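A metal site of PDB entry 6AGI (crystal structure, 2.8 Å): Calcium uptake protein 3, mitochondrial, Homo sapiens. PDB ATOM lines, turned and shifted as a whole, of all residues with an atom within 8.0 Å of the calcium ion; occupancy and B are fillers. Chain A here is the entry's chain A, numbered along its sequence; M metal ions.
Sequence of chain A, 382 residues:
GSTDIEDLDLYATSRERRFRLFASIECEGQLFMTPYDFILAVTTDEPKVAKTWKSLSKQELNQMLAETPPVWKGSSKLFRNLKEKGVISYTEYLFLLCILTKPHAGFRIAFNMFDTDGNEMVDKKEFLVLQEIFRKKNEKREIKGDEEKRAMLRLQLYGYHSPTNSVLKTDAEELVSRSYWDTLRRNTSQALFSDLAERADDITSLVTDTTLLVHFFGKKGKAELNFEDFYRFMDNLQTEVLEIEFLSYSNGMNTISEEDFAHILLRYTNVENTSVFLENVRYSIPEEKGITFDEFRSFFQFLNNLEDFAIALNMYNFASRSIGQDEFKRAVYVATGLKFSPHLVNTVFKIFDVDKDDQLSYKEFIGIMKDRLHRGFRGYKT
OE2 of Glu 126 sits close to N of Thr 116 (3.1 Å).
The backbone NH of Glu 120 sits at hydrogen-bond distance from the side-chain carboxylate of Asp 115, at 2.8 Å.
OE1 of Glu 126 lies close to N of Asp 123 (2.7 Å).
The side-chain carboxylate of Asp 115 sits close to the backbone NH of Gly 118, 3.2 Å away.
Residues that only touch the calcium ion: Asp 123 (3.6 Å).
Of the 16 residues printed, 6 come within 4 Å of the calcium ion.
The calcium ion is bound by OD1 of Asn 119 (2.4 Å), OD1 of Asp 115 (2.4 Å), O of Met 121 (2.5 Å), OE1 of Glu 126 (2.6 Å), OE2 of Glu 126 (2.6 Å) and OD1 of Asp 117 (2.8 Å).
Slightly farther from the calcium ion lies OD2 of Asp 117 (3.1 Å).
Slightly farther from the calcium ion lies the side-chain amide nitrogen (ND2) of Asn 119 (3.1 Å).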
ATOM      1  N   PHE A 111     -12.823 -12.471  -1.189  1.00  0.00           N
ATOM      2  CA  PHE A 111     -12.812 -13.889  -0.903  1.00  0.00           C
ATOM      3  C   PHE A 111     -14.203 -14.378  -0.477  1.00  0.00           C
ATOM      4  O   PHE A 111     -14.738 -15.363  -1.020  1.00  0.00           O
ATOM      5  CB  PHE A 111     -11.777 -14.161   0.192  1.00  0.00           C
ATOM      6  CG  PHE A 111     -11.557 -15.612   0.498  1.00  0.00           C
ATOM      7  CD1 PHE A 111     -10.675 -16.369  -0.250  1.00  0.00           C
ATOM      8  CD2 PHE A 111     -12.245 -16.237   1.546  1.00  0.00           C
ATOM      9  CE1 PHE A 111     -10.476 -17.716   0.027  1.00  0.00           C
ATOM     10  CE2 PHE A 111     -12.055 -17.582   1.827  1.00  0.00           C
ATOM     11  CZ  PHE A 111     -11.164 -18.319   1.069  1.00  0.00           C
ATOM     12  N   PHE A 114     -16.666 -14.725  -3.069  1.00  0.00           N
ATOM     13  CA  PHE A 114     -16.541 -15.958  -3.864  1.00  0.00           C
ATOM     14  C   PHE A 114     -17.093 -17.185  -3.141  1.00  0.00           C
ATOM     15  O   PHE A 114     -17.720 -18.042  -3.771  1.00  0.00           O
ATOM     16  CB  PHE A 114     -15.079 -16.217  -4.229  1.00  0.00           C
ATOM     17  CG  PHE A 114     -14.608 -15.502  -5.464  1.00  0.00           C
ATOM     18  CD1 PHE A 114     -14.966 -15.945  -6.719  1.00  0.00           C
ATOM     19  CD2 PHE A 114     -13.728 -14.423  -5.363  1.00  0.00           C
ATOM     20  CE1 PHE A 114     -14.505 -15.292  -7.866  1.00  0.00           C
ATOM     21  CE2 PHE A 114     -13.259 -13.778  -6.490  1.00  0.00           C
ATOM     22  CZ  PHE A 114     -13.647 -14.202  -7.745  1.00  0.00           C
ATOM     23  N   ASP A 115     -16.874 -17.307  -1.826  1.00  0.00           N
ATOM     24  CA  ASP A 115     -17.153 -18.513  -1.041  1.00  0.00           C
ATOM     25  C   ASP A 115     -18.648 -18.599  -0.723  1.00  0.00           C
ATOM     26  O   ASP A 115     -19.085 -18.433   0.416  1.00  0.00           O
ATOM     27  CB  ASP A 115     -16.304 -18.504   0.224  1.00  0.00           C
ATOM     28  CG  ASP A 115     -16.396 -19.804   1.028  1.00  0.00           C
ATOM     29  OD1 ASP A 115     -16.782 -20.848   0.462  1.00  0.00           O
ATOM     30  OD2 ASP A 115     -16.052 -19.774   2.229  1.00  0.00           O
ATOM     31  N   THR A 116     -19.421 -18.897  -1.769  1.00  0.00           N
ATOM     32  CA  THR A 116     -20.873 -19.063  -1.653  1.00  0.00           C
ATOM     33  C   THR A 116     -21.290 -19.980  -0.516  1.00  0.00           C
ATOM     34  O   THR A 116     -22.353 -19.768   0.091  1.00  0.00           O
ATOM     35  CB  THR A 116     -21.448 -19.594  -2.973  1.00  0.00           C
ATOM     36  OG1 THR A 116     -20.955 -20.925  -3.214  1.00  0.00           O
ATOM     37  CG2 THR A 116     -21.076 -18.691  -4.128  1.00  0.00           C
ATOM     38  N   ASP A 117     -20.501 -21.012  -0.201  1.00  0.00           N
ATOM     39  CA  ASP A 117     -20.952 -22.003   0.781  1.00  0.00           C
ATOM     40  C   ASP A 117     -20.339 -21.843   2.158  1.00  0.00           C
ATOM     41  O   ASP A 117     -20.744 -22.556   3.075  1.00  0.00           O
ATOM     42  CB  ASP A 117     -20.689 -23.428   0.316  1.00  0.00           C
ATOM     43  CG  ASP A 117     -19.274 -23.637  -0.134  1.00  0.00           C
ATOM     44  OD1 ASP A 117     -18.937 -23.158  -1.224  1.00  0.00           O
ATOM     45  OD2 ASP A 117     -18.494 -24.236   0.629  1.00  0.00           O
ATOM     46  N   GLY A 118     -19.335 -20.983   2.324  1.00  0.00           N
ATOM     47  CA  GLY A 118     -18.912 -20.643   3.673  1.00  0.00           C
ATOM     48  C   GLY A 118     -17.884 -21.553   4.306  1.00  0.00           C
ATOM     49  O   GLY A 118     -17.535 -21.331   5.479  1.00  0.00           O
ATOM     50  N   ASN A 119     -17.418 -22.596   3.610  1.00  0.00           N
ATOM     51  CA  ASN A 119     -16.389 -23.492   4.132  1.00  0.00           C
ATOM     52  C   ASN A 119     -15.010 -22.834   4.318  1.00  0.00           C
ATOM     53  O   ASN A 119     -14.093 -23.542   4.783  1.00  0.00           O
ATOM     54  CB  ASN A 119     -16.252 -24.713   3.222  1.00  0.00           C
ATOM     55  CG  ASN A 119     -15.849 -24.345   1.806  1.00  0.00           C
ATOM     56  OD1 ASN A 119     -15.635 -23.163   1.502  1.00  0.00           O
ATOM     57  ND2 ASN A 119     -15.760 -25.343   0.936  1.00  0.00           N
ATOM     58  N   GLU A 120     -14.834 -21.554   3.953  1.00  0.00           N
ATOM     59  CA  GLU A 120     -13.573 -20.806   4.014  1.00  0.00           C
ATOM     60  C   GLU A 120     -12.543 -21.251   2.971  1.00  0.00           C
ATOM     61  O   GLU A 120     -11.359 -20.943   3.109  1.00  0.00           O
ATOM     62  CB  GLU A 120     -12.910 -20.890   5.388  1.00  0.00           C
ATOM     63  CG  GLU A 120     -13.353 -19.893   6.433  1.00  0.00           C
ATOM     64  CD  GLU A 120     -13.142 -20.435   7.840  1.00  0.00           C
ATOM     65  OE1 GLU A 120     -12.617 -21.562   7.955  1.00  0.00           O
ATOM     66  OE2 GLU A 120     -13.422 -19.693   8.817  1.00  0.00           O
ATOM     67  N   MET A 121     -12.963 -21.963   1.924  1.00  0.00           N
ATOM     68  CA  MET A 121     -12.155 -22.223   0.743  1.00  0.00           C
ATOM     69  C   MET A 121     -12.923 -21.800  -0.498  1.00  0.00           C
ATOM     70  O   MET A 121     -14.114 -21.478  -0.444  1.00  0.00           O
ATOM     71  CB  MET A 121     -11.760 -23.717   0.626  1.00  0.00           C
ATOM     72  CG  MET A 121     -11.274 -24.389   1.902  1.00  0.00           C
ATOM     73  SD  MET A 121      -9.698 -23.782   2.516  1.00  0.00           S
ATOM     74  CE  MET A 121      -8.744 -25.299   2.460  1.00  0.00           C
ATOM     75  N   VAL A 122     -12.223 -21.765  -1.627  1.00  0.00           N
ATOM     76  CA  VAL A 122     -12.794 -21.380  -2.913  1.00  0.00           C
ATOM     77  C   VAL A 122     -12.556 -22.524  -3.892  1.00  0.00           C
ATOM     78  O   VAL A 122     -11.411 -22.791  -4.275  1.00  0.00           O
ATOM     79  CB  VAL A 122     -12.198 -20.066  -3.422  1.00  0.00           C
ATOM     80  CG1 VAL A 122     -12.639 -19.766  -4.850  1.00  0.00           C
ATOM     81  CG2 VAL A 122     -12.605 -18.917  -2.509  1.00  0.00           C
ATOM     82  N   ASP A 123     -13.628 -23.202  -4.295  1.00  0.00           N
ATOM     83  CA  ASP A 123     -13.600 -24.191  -5.356  1.00  0.00           C
ATOM     84  C   ASP A 123     -13.188 -23.531  -6.667  1.00  0.00           C
ATOM     85  O   ASP A 123     -13.395 -22.326  -6.871  1.00  0.00           O
ATOM     86  CB  ASP A 123     -14.981 -24.799  -5.608  1.00  0.00           C
ATOM     87  CG  ASP A 123     -15.684 -25.227  -4.340  1.00  0.00           C
ATOM     88  OD1 ASP A 123     -15.050 -25.215  -3.254  1.00  0.00           O
ATOM     89  OD2 ASP A 123     -16.896 -25.524  -4.424  1.00  0.00           O
ATOM     90  N   LYS A 124     -12.704 -24.341  -7.601  1.00  0.00           N
ATOM     91  CA  LYS A 124     -12.640 -23.849  -8.965  1.00  0.00           C
ATOM     92  C   LYS A 124     -13.994 -23.352  -9.442  1.00  0.00           C
ATOM     93  O   LYS A 124     -14.087 -22.317 -10.104  1.00  0.00           O
ATOM     94  CB  LYS A 124     -12.134 -24.927  -9.906  1.00  0.00           C
ATOM     95  CG  LYS A 124     -11.934 -24.413 -11.321  1.00  0.00           C
ATOM     96  CD  LYS A 124     -11.298 -25.462 -12.237  1.00  0.00           C
ATOM     97  CE  LYS A 124     -11.450 -25.065 -13.707  1.00  0.00           C
ATOM     98  NZ  LYS A 124     -10.529 -25.836 -14.594  1.00  0.00           N
ATOM     99  N   LYS A 125     -15.062 -24.035  -9.033  1.00  0.00           N
ATOM    100  CA  LYS A 125     -16.372 -23.768  -9.620  1.00  0.00           C
ATOM    101  C   LYS A 125     -17.055 -22.563  -8.978  1.00  0.00           C
ATOM    102  O   LYS A 125     -17.839 -21.870  -9.645  1.00  0.00           O
ATOM    103  CB  LYS A 125     -17.257 -25.010  -9.501  1.00  0.00           C
ATOM    104  CG  LYS A 125     -18.684 -24.838 -10.021  1.00  0.00           C
ATOM    105  CD  LYS A 125     -19.696 -25.126  -8.914  1.00  0.00           C
ATOM    106  CE  LYS A 125     -19.999 -23.858  -8.100  1.00  0.00           C
ATOM    107  NZ  LYS A 125     -20.641 -24.217  -6.802  1.00  0.00           N
ATOM    108  N   GLU A 126     -16.784 -22.270  -7.714  1.00  0.00           N
ATOM    109  CA  GLU A 126     -17.107 -20.951  -7.179  1.00  0.00           C
ATOM    110  C   GLU A 126     -16.516 -19.830  -8.039  1.00  0.00           C
ATOM    111  O   GLU A 126     -17.220 -18.906  -8.508  1.00  0.00           O
ATOM    112  CB  GLU A 126     -16.602 -20.866  -5.746  1.00  0.00           C
ATOM    113  CG  GLU A 126     -17.599 -21.465  -4.757  1.00  0.00           C
ATOM    114  CD  GLU A 126     -17.019 -21.671  -3.374  1.00  0.00           C
ATOM    115  OE1 GLU A 126     -15.847 -22.048  -3.249  1.00  0.00           O
ATOM    116  OE2 GLU A 126     -17.737 -21.390  -2.403  1.00  0.00           O
ATOM    117  N   GLU A 224      -8.376 -26.507  -3.787  1.00  0.00           N
ATOM    118  CA  GLU A 224      -9.163 -25.330  -3.475  1.00  0.00           C
ATOM    119  C   GLU A 224      -8.281 -24.363  -2.734  1.00  0.00           C
ATOM    120  O   GLU A 224      -7.216 -24.721  -2.222  1.00  0.00           O
ATOM    121  CB  GLU A 224     -10.443 -25.620  -2.694  1.00  0.00           C
ATOM    122  CG  GLU A 224     -10.428 -26.785  -1.766  1.00  0.00           C
ATOM    123  CD  GLU A 224     -11.834 -27.150  -1.363  1.00  0.00           C
ATOM    124  OE1 GLU A 224     -12.007 -27.784  -0.303  1.00  0.00           O
ATOM    125  OE2 GLU A 224     -12.783 -26.796  -2.092  1.00  0.00           O
ATOM    126  N   LEU A 225      -8.724 -23.127  -2.700  1.00  0.00           N
ATOM    127  CA  LEU A 225      -7.904 -22.001  -2.352  1.00  0.00           C
ATOM    128  C   LEU A 225      -8.312 -21.481  -0.979  1.00  0.00           C
ATOM    129  O   LEU A 225      -9.468 -21.055  -0.800  1.00  0.00           O
ATOM    130  CB  LEU A 225      -8.044 -20.946  -3.447  1.00  0.00           C
ATOM    131  CG  LEU A 225      -7.458 -19.535  -3.539  1.00  0.00           C
ATOM    132  CD1 LEU A 225      -5.932 -19.423  -3.269  1.00  0.00           C
ATOM    133  CD2 LEU A 225      -7.802 -19.029  -4.929  1.00  0.00           C
HETATM  134 CA    CA M   1     -16.184 -22.837  -0.836  1.00  0.00          CA
